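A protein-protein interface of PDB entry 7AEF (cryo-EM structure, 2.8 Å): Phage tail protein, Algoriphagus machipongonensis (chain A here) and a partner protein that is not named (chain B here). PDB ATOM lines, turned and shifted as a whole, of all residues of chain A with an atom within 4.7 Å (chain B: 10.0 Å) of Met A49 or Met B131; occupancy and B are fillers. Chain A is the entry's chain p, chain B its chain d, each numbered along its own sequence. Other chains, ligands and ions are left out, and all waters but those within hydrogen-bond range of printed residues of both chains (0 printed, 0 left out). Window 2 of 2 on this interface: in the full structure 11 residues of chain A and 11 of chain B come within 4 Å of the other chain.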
ATOM      1  N   GLU A  32     -23.184 -31.230   2.888  1.00  0.00           N
ATOM      2  CA  GLU A  32     -23.243 -32.023   4.125  1.00  0.00           C
ATOM      3  C   GLU A  32     -23.699 -31.228   5.347  1.00  0.00           C
ATOM      4  O   GLU A  32     -23.589 -30.001   5.385  1.00  0.00           O
ATOM      5  CB  GLU A  32     -21.871 -32.605   4.437  1.00  0.00           C
ATOM      6  CG  GLU A  32     -21.390 -33.621   3.468  1.00  0.00           C
ATOM      7  CD  GLU A  32     -22.176 -34.865   3.573  1.00  0.00           C
ATOM      8  OE1 GLU A  32     -22.479 -35.251   4.668  1.00  0.00           O
ATOM      9  OE2 GLU A  32     -22.501 -35.441   2.566  1.00  0.00           O
ATOM     10  N   ILE A  33     -24.205 -31.933   6.355  1.00  0.00           N
ATOM     11  CA  ILE A  33     -24.689 -31.273   7.563  1.00  0.00           C
ATOM     12  C   ILE A  33     -23.970 -31.691   8.846  1.00  0.00           C
ATOM     13  O   ILE A  33     -23.804 -32.880   9.126  1.00  0.00           O
ATOM     14  CB  ILE A  33     -26.202 -31.491   7.750  1.00  0.00           C
ATOM     15  CG1 ILE A  33     -26.966 -31.025   6.509  1.00  0.00           C
ATOM     16  CG2 ILE A  33     -26.696 -30.759   8.989  1.00  0.00           C
ATOM     17  CD1 ILE A  33     -28.464 -31.209   6.608  1.00  0.00           C
ATOM     18  N   ILE A  34     -23.551 -30.694   9.618  1.00  0.00           N
ATOM     19  CA  ILE A  34     -22.887 -30.903  10.893  1.00  0.00           C
ATOM     20  C   ILE A  34     -23.878 -30.636  12.034  1.00  0.00           C
ATOM     21  O   ILE A  34     -24.497 -29.574  12.093  1.00  0.00           O
ATOM     22  CB  ILE A  34     -21.659 -29.991  11.008  1.00  0.00           C
ATOM     23  CG1 ILE A  34     -20.683 -30.322   9.865  1.00  0.00           C
ATOM     24  CG2 ILE A  34     -21.006 -30.174  12.381  1.00  0.00           C
ATOM     25  CD1 ILE A  34     -19.586 -29.332   9.671  1.00  0.00           C
ATOM     26  N   TYR A  36     -25.080 -30.635  16.307  1.00  0.00           N
ATOM     27  CA  TYR A  36     -24.572 -30.437  17.681  1.00  0.00           C
ATOM     28  C   TYR A  36     -25.618 -30.235  18.800  1.00  0.00           C
ATOM     29  O   TYR A  36     -26.654 -29.603  18.601  1.00  0.00           O
ATOM     30  CB  TYR A  36     -23.649 -29.208  17.664  1.00  0.00           C
ATOM     31  CG  TYR A  36     -22.993 -28.832  18.978  1.00  0.00           C
ATOM     32  CD1 TYR A  36     -21.824 -29.437  19.368  1.00  0.00           C
ATOM     33  CD2 TYR A  36     -23.569 -27.874  19.790  1.00  0.00           C
ATOM     34  CE1 TYR A  36     -21.233 -29.081  20.553  1.00  0.00           C
ATOM     35  CE2 TYR A  36     -22.981 -27.523  20.970  1.00  0.00           C
ATOM     36  CZ  TYR A  36     -21.817 -28.118  21.353  1.00  0.00           C
ATOM     37  OH  TYR A  36     -21.222 -27.765  22.533  1.00  0.00           O
ATOM     38  N   ILE A  47     -28.855 -28.807  16.787  1.00  0.00           N
ATOM     39  CA  ILE A  47     -28.741 -27.625  15.931  1.00  0.00           C
ATOM     40  C   ILE A  47     -27.903 -27.990  14.712  1.00  0.00           C
ATOM     41  O   ILE A  47     -26.970 -28.791  14.803  1.00  0.00           O
ATOM     42  CB  ILE A  47     -28.177 -26.386  16.668  1.00  0.00           C
ATOM     43  CG1 ILE A  47     -26.743 -26.634  17.200  1.00  0.00           C
ATOM     44  CG2 ILE A  47     -29.136 -26.040  17.801  1.00  0.00           C
ATOM     45  CD1 ILE A  47     -26.022 -25.417  17.703  1.00  0.00           C
ATOM     46  N   LYS A  48     -28.275 -27.469  13.543  1.00  0.00           N
ATOM     47  CA  LYS A  48     -27.585 -27.841  12.307  1.00  0.00           C
ATOM     48  C   LYS A  48     -26.863 -26.711  11.569  1.00  0.00           C
ATOM     49  O   LYS A  48     -27.384 -25.602  11.462  1.00  0.00           O
ATOM     50  CB  LYS A  48     -28.653 -28.416  11.393  1.00  0.00           C
ATOM     51  CG  LYS A  48     -29.323 -29.619  11.988  1.00  0.00           C
ATOM     52  CD  LYS A  48     -30.399 -30.184  11.133  1.00  0.00           C
ATOM     53  CE  LYS A  48     -31.058 -31.349  11.840  1.00  0.00           C
ATOM     54  NZ  LYS A  48     -32.152 -31.936  11.048  1.00  0.00           N
ATOM     55  N   MET A  49     -25.703 -27.027  10.979  1.00  0.00           N
ATOM     56  CA  MET A  49     -24.992 -26.062  10.130  1.00  0.00           C
ATOM     57  C   MET A  49     -24.336 -26.746   8.906  1.00  0.00           C
ATOM     58  O   MET A  49     -24.005 -27.927   8.975  1.00  0.00           O
ATOM     59  CB  MET A  49     -23.932 -25.315  10.938  1.00  0.00           C
ATOM     60  CG  MET A  49     -22.811 -26.158  11.452  1.00  0.00           C
ATOM     61  SD  MET A  49     -21.647 -25.213  12.430  1.00  0.00           S
ATOM     62  CE  MET A  49     -20.392 -26.434  12.716  1.00  0.00           C
ATOM     63  N   PRO A  50     -24.115 -26.039   7.779  1.00  0.00           N
ATOM     64  CA  PRO A  50     -23.423 -26.518   6.585  1.00  0.00           C
ATOM     65  C   PRO A  50     -21.985 -27.003   6.765  1.00  0.00           C
ATOM     66  O   PRO A  50     -21.176 -26.352   7.424  1.00  0.00           O
ATOM     67  CB  PRO A  50     -23.393 -25.262   5.712  1.00  0.00           C
ATOM     68  CG  PRO A  50     -24.538 -24.443   6.161  1.00  0.00           C
ATOM     69  CD  PRO A  50     -24.630 -24.662   7.634  1.00  0.00           C
ATOM     70  N   GLY A  51     -21.695 -28.103   6.090  1.00  0.00           N
ATOM     71  CA  GLY A  51     -20.419 -28.797   5.969  1.00  0.00           C
ATOM     72  C   GLY A  51     -19.802 -28.608   4.579  1.00  0.00           C
ATOM     73  O   GLY A  51     -19.976 -27.574   3.932  1.00  0.00           O
ATOM     74  N   GLN B  29     -20.617 -30.919  26.029  1.00  0.00           N
ATOM     75  CA  GLN B  29     -21.029 -32.084  25.251  1.00  0.00           C
ATOM     76  C   GLN B  29     -21.025 -33.362  26.087  1.00  0.00           C
ATOM     77  O   GLN B  29     -21.913 -34.215  25.926  1.00  0.00           O
ATOM     78  CB  GLN B  29     -20.099 -32.245  24.044  1.00  0.00           C
ATOM     79  CG  GLN B  29     -20.388 -33.468  23.197  1.00  0.00           C
ATOM     80  CD  GLN B  29     -19.433 -33.622  22.035  1.00  0.00           C
ATOM     81  OE1 GLN B  29     -18.572 -32.777  21.812  1.00  0.00           O
ATOM     82  NE2 GLN B  29     -19.585 -34.706  21.286  1.00  0.00           N
ATOM     83  N   LYS B  67     -15.789 -32.291  27.780  1.00  0.00           N
ATOM     84  CA  LYS B  67     -15.658 -32.021  26.343  1.00  0.00           C
ATOM     85  C   LYS B  67     -16.723 -31.063  25.821  1.00  0.00           C
ATOM     86  O   LYS B  67     -17.856 -31.051  26.306  1.00  0.00           O
ATOM     87  CB  LYS B  67     -15.741 -33.292  25.515  1.00  0.00           C
ATOM     88  CG  LYS B  67     -14.600 -34.226  25.720  1.00  0.00           C
ATOM     89  CD  LYS B  67     -14.723 -35.418  24.816  1.00  0.00           C
ATOM     90  CE  LYS B  67     -13.566 -36.373  25.006  1.00  0.00           C
ATOM     91  NZ  LYS B  67     -13.712 -37.599  24.168  1.00  0.00           N
ATOM     92  N   ARG B  68     -16.350 -30.291  24.791  1.00  0.00           N
ATOM     93  CA  ARG B  68     -17.238 -29.339  24.117  1.00  0.00           C
ATOM     94  C   ARG B  68     -16.645 -28.879  22.786  1.00  0.00           C
ATOM     95  O   ARG B  68     -15.472 -29.114  22.506  1.00  0.00           O
ATOM     96  CB  ARG B  68     -17.477 -28.122  24.986  1.00  0.00           C
ATOM     97  CG  ARG B  68     -16.225 -27.334  25.199  1.00  0.00           C
ATOM     98  CD  ARG B  68     -16.483 -26.163  26.015  1.00  0.00           C
ATOM     99  NE  ARG B  68     -15.286 -25.360  26.093  1.00  0.00           N
ATOM    100  CZ  ARG B  68     -15.142 -24.289  26.854  1.00  0.00           C
ATOM    101  NH1 ARG B  68     -16.119 -23.865  27.642  1.00  0.00           N
ATOM    102  NH2 ARG B  68     -13.997 -23.647  26.801  1.00  0.00           N
ATOM    103  N   GLY B  69     -17.452 -28.177  21.982  1.00  0.00           N
ATOM    104  CA  GLY B  69     -16.916 -27.533  20.787  1.00  0.00           C
ATOM    105  C   GLY B  69     -16.015 -26.377  21.174  1.00  0.00           C
ATOM    106  O   GLY B  69     -16.196 -25.774  22.221  1.00  0.00           O
ATOM    107  N   VAL B  70     -15.043 -26.044  20.314  1.00  0.00           N
ATOM    108  CA  VAL B  70     -14.071 -24.988  20.635  1.00  0.00           C
ATOM    109  C   VAL B  70     -14.716 -23.618  20.846  1.00  0.00           C
ATOM    110  O   VAL B  70     -15.461 -23.116  19.998  1.00  0.00           O
ATOM    111  CB  VAL B  70     -13.006 -24.885  19.533  1.00  0.00           C
ATOM    112  CG1 VAL B  70     -12.116 -23.658  19.734  1.00  0.00           C
ATOM    113  CG2 VAL B  70     -12.132 -26.110  19.527  1.00  0.00           C
ATOM    114  N   LEU B  71     -14.379 -22.993  21.977  1.00  0.00           N
ATOM    115  CA  LEU B  71     -14.806 -21.653  22.359  1.00  0.00           C
ATOM    116  C   LEU B  71     -13.556 -20.801  22.532  1.00  0.00           C
ATOM    117  O   LEU B  71     -12.672 -21.159  23.311  1.00  0.00           O
ATOM    118  CB  LEU B  71     -15.613 -21.698  23.664  1.00  0.00           C
ATOM    119  CG  LEU B  71     -16.092 -20.377  24.284  1.00  0.00           C
ATOM    120  CD1 LEU B  71     -17.089 -19.684  23.374  1.00  0.00           C
ATOM    121  CD2 LEU B  71     -16.715 -20.637  25.655  1.00  0.00           C
ATOM    122  N   VAL B 121      -6.858 -30.158  21.728  1.00  0.00           N
ATOM    123  CA  VAL B 121      -7.826 -29.965  20.654  1.00  0.00           C
ATOM    124  C   VAL B 121      -7.551 -31.064  19.624  1.00  0.00           C
ATOM    125  O   VAL B 121      -6.391 -31.354  19.314  1.00  0.00           O
ATOM    126  CB  VAL B 121      -7.717 -28.561  20.013  1.00  0.00           C
ATOM    127  CG1 VAL B 121      -8.603 -28.442  18.768  1.00  0.00           C
ATOM    128  CG2 VAL B 121      -8.018 -27.490  21.021  1.00  0.00           C
ATOM    129  N   GLU B 122      -8.614 -31.689  19.116  1.00  0.00           N
ATOM    130  CA  GLU B 122      -8.498 -32.795  18.170  1.00  0.00           C
ATOM    131  C   GLU B 122      -7.956 -32.363  16.803  1.00  0.00           C
ATOM    132  O   GLU B 122      -8.112 -31.218  16.379  1.00  0.00           O
ATOM    133  CB  GLU B 122      -9.854 -33.480  17.997  1.00  0.00           C
ATOM    134  CG  GLU B 122     -10.320 -34.172  19.259  1.00  0.00           C
ATOM    135  CD  GLU B 122     -11.550 -34.999  19.075  1.00  0.00           C
ATOM    136  OE1 GLU B 122     -12.138 -34.955  17.997  1.00  0.00           O
ATOM    137  OE2 GLU B 122     -11.987 -35.624  20.047  1.00  0.00           O
ATOM    138  N   ASP B 123      -7.343 -33.330  16.108  1.00  0.00           N
ATOM    139  CA  ASP B 123      -6.666 -33.156  14.819  1.00  0.00           C
ATOM    140  C   ASP B 123      -7.542 -32.548  13.726  1.00  0.00           C
ATOM    141  O   ASP B 123      -8.731 -32.845  13.599  1.00  0.00           O
ATOM    142  CB  ASP B 123      -6.204 -34.498  14.261  1.00  0.00           C
ATOM    143  CG  ASP B 123      -5.072 -35.125  15.018  1.00  0.00           C
ATOM    144  OD1 ASP B 123      -4.485 -34.514  15.900  1.00  0.00           O
ATOM    145  OD2 ASP B 123      -4.766 -36.276  14.707  1.00  0.00           O
ATOM    146  N   PHE B 124      -6.901 -31.763  12.879  1.00  0.00           N
ATOM    147  CA  PHE B 124      -7.536 -31.139  11.736  1.00  0.00           C
ATOM    148  C   PHE B 124      -7.414 -32.069  10.538  1.00  0.00           C
ATOM    149  O   PHE B 124      -6.405 -32.753  10.388  1.00  0.00           O
ATOM    150  CB  PHE B 124      -6.860 -29.808  11.426  1.00  0.00           C
ATOM    151  CG  PHE B 124      -6.941 -28.783  12.538  1.00  0.00           C
ATOM    152  CD1 PHE B 124      -6.052 -27.736  12.544  1.00  0.00           C
ATOM    153  CD2 PHE B 124      -7.879 -28.854  13.566  1.00  0.00           C
ATOM    154  CE1 PHE B 124      -6.086 -26.783  13.537  1.00  0.00           C
ATOM    155  CE2 PHE B 124      -7.903 -27.908  14.563  1.00  0.00           C
ATOM    156  CZ  PHE B 124      -7.009 -26.869  14.541  1.00  0.00           C
ATOM    157  N   ASN B 125      -8.436 -32.090   9.685  1.00  0.00           N
ATOM    158  CA  ASN B 125      -8.399 -32.944   8.497  1.00  0.00           C
ATOM    159  C   ASN B 125      -9.122 -32.247   7.352  1.00  0.00           C
ATOM    160  O   ASN B 125     -10.339 -32.078   7.380  1.00  0.00           O
ATOM    161  CB  ASN B 125      -9.002 -34.309   8.795  1.00  0.00           C
ATOM    162  CG  ASN B 125      -8.834 -35.306   7.655  1.00  0.00           C
ATOM    163  OD1 ASN B 125      -8.790 -34.981   6.464  1.00  0.00           O
ATOM    164  ND2 ASN B 125      -8.749 -36.555   8.032  1.00  0.00           N
ATOM    165  N   GLU B 128     -12.332 -34.037   5.713  1.00  0.00           N
ATOM    166  CA  GLU B 128     -13.474 -34.507   6.480  1.00  0.00           C
ATOM    167  C   GLU B 128     -14.319 -33.323   6.948  1.00  0.00           C
ATOM    168  O   GLU B 128     -13.800 -32.251   7.251  1.00  0.00           O
ATOM    169  CB  GLU B 128     -13.003 -35.277   7.699  1.00  0.00           C
ATOM    170  CG  GLU B 128     -12.398 -36.628   7.402  1.00  0.00           C
ATOM    171  CD  GLU B 128     -12.011 -37.349   8.663  1.00  0.00           C
ATOM    172  OE1 GLU B 128     -11.792 -36.688   9.679  1.00  0.00           O
ATOM    173  OE2 GLU B 128     -11.981 -38.584   8.662  1.00  0.00           O
ATOM    174  N   SER B 129     -15.618 -33.517   7.022  1.00  0.00           N
ATOM    175  CA  SER B 129     -16.532 -32.521   7.577  1.00  0.00           C
ATOM    176  C   SER B 129     -16.807 -32.759   9.042  1.00  0.00           C
ATOM    177  O   SER B 129     -17.605 -33.626   9.393  1.00  0.00           O
ATOM    178  CB  SER B 129     -17.831 -32.520   6.799  1.00  0.00           C
ATOM    179  OG  SER B 129     -18.653 -31.474   7.240  1.00  0.00           O
ATOM    180  N   LYS B 130     -16.142 -31.989   9.909  1.00  0.00           N
ATOM    181  CA  LYS B 130     -16.208 -32.189  11.350  1.00  0.00           C
ATOM    182  C   LYS B 130     -16.087 -30.874  12.106  1.00  0.00           C
ATOM    183  O   LYS B 130     -15.525 -29.898  11.612  1.00  0.00           O
ATOM    184  CB  LYS B 130     -15.095 -33.126  11.806  1.00  0.00           C
ATOM    185  CG  LYS B 130     -15.286 -34.568  11.434  1.00  0.00           C
ATOM    186  CD  LYS B 130     -14.193 -35.434  11.965  1.00  0.00           C
ATOM    187  CE  LYS B 130     -14.349 -36.862  11.469  1.00  0.00           C
ATOM    188  NZ  LYS B 130     -13.185 -37.712  11.849  1.00  0.00           N
ATOM    189  N   MET B 131     -16.592 -30.879  13.332  1.00  0.00           N
ATOM    190  CA  MET B 131     -16.480 -29.750  14.244  1.00  0.00           C
ATOM    191  C   MET B 131     -15.177 -29.840  15.022  1.00  0.00           C
ATOM    192  O   MET B 131     -14.742 -30.931  15.378  1.00  0.00           O
ATOM    193  CB  MET B 131     -17.665 -29.759  15.203  1.00  0.00           C
ATOM    194  CG  MET B 131     -17.710 -28.616  16.176  1.00  0.00           C
ATOM    195  SD  MET B 131     -19.152 -28.666  17.216  1.00  0.00           S
ATOM    196  CE  MET B 131     -20.431 -28.111  16.102  1.00  0.00           C
ATOM    197  N   ALA B 132     -14.556 -28.698  15.301  1.00  0.00           N
ATOM    198  CA  ALA B 132     -13.374 -28.708  16.150  1.00  0.00           C
ATOM    199  C   ALA B 132     -13.782 -28.910  17.603  1.00  0.00           C
ATOM    200  O   ALA B 132     -14.589 -28.146  18.137  1.00  0.00           O
ATOM    201  CB  ALA B 132     -12.584 -27.416  15.996  1.00  0.00           C
ATOM    202  N   ILE B 133     -13.204 -29.931  18.241  1.00  0.00           N
ATOM    203  CA  ILE B 133     -13.555 -30.325  19.604  1.00  0.00           C
ATOM    204  C   ILE B 133     -12.402 -30.097  20.576  1.00  0.00           C
ATOM    205  O   ILE B 133     -11.253 -30.496  20.325  1.00  0.00           O
ATOM    206  CB  ILE B 133     -14.034 -31.786  19.666  1.00  0.00           C
ATOM    207  CG1 ILE B 133     -15.247 -31.999  18.733  1.00  0.00           C
ATOM    208  CG2 ILE B 133     -14.356 -32.222  21.111  1.00  0.00           C
ATOM    209  CD1 ILE B 133     -16.488 -31.151  19.019  1.00  0.00           C
ATOM    210  N   GLU B 134     -12.748 -29.495  21.717  1.00  0.00           N
ATOM    211  CA  GLU B 134     -11.821 -29.176  22.784  1.00  0.00           C
ATOM    212  C   GLU B 134     -12.052 -30.097  23.992  1.00  0.00           C
ATOM    213  O   GLU B 134     -13.187 -30.483  24.302  1.00  0.00           O
ATOM    214  CB  GLU B 134     -11.976 -27.707  23.145  1.00  0.00           C
ATOM    215  CG  GLU B 134     -11.278 -27.261  24.358  1.00  0.00           C
ATOM    216  CD  GLU B 134     -11.341 -25.804  24.445  1.00  0.00           C
ATOM    217  OE1 GLU B 134     -12.415 -25.303  24.779  1.00  0.00           O
ATOM    218  OE2 GLU B 134     -10.298 -25.161  24.374  1.00  0.00           O
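Printed residues of chain B that touch a printed residue of chain A: Gly B69, Ser B129 and Met B131. Among the printed residues, 5 pairs touch across the chains. Among the printed residues, no Asp or Glu carboxylate lies within 4 Å of a Lys or Arg side-chain nitrogen of the other chain.
The backbone carbonyl oxygen of Tyr A36 sits at hydrogen-bond distance from the backbone NH of Ile A47 (3.0 Å). O of Met A49 sits at hydrogen-bond distance from N of Ile A34 (2.9 Å). The backbone carbonyl oxygen (O) of Glu A32 is in hydrogen-bond range of the backbone NH (N) of Gly A51, 2.8 Å away.
CD1 of Ile A34 touches OG of Ser B129, at 3.4 Å. N of Gly B69 touches OH of Tyr A36 (3.8 Å). CD1 of Tyr A36 touches SD of Met B131 (3.5 Å). Met A49 touches Met B131 (CE to CE, 3.8 Å). OG of Ser B129 touches CA of Gly A51 (3.4 Å).
Of chain B, only Met B131 comes within 4 Å of Met A49. No residue of chain B comes within 4 Å of Pro A50. Of the printed residues of chain B, Tyr A36 touches Gly B69 (3.8 Å) and Met B131 (3.5 Å). Printed residues of chain A within 4 Å of Gly B69: Tyr A36. Of the printed residues of chain A, Ser B129 touches Ile A34 (3.4 Å) and Gly A51 (3.4 Å). Of the printed residues of chain B, Gly A51 touches Ser B129. Glu A32 touches none of the printed residues of chain B. The nearest residue of chain B that does not touch Met A49 is Lys B130 (6.1 Å).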
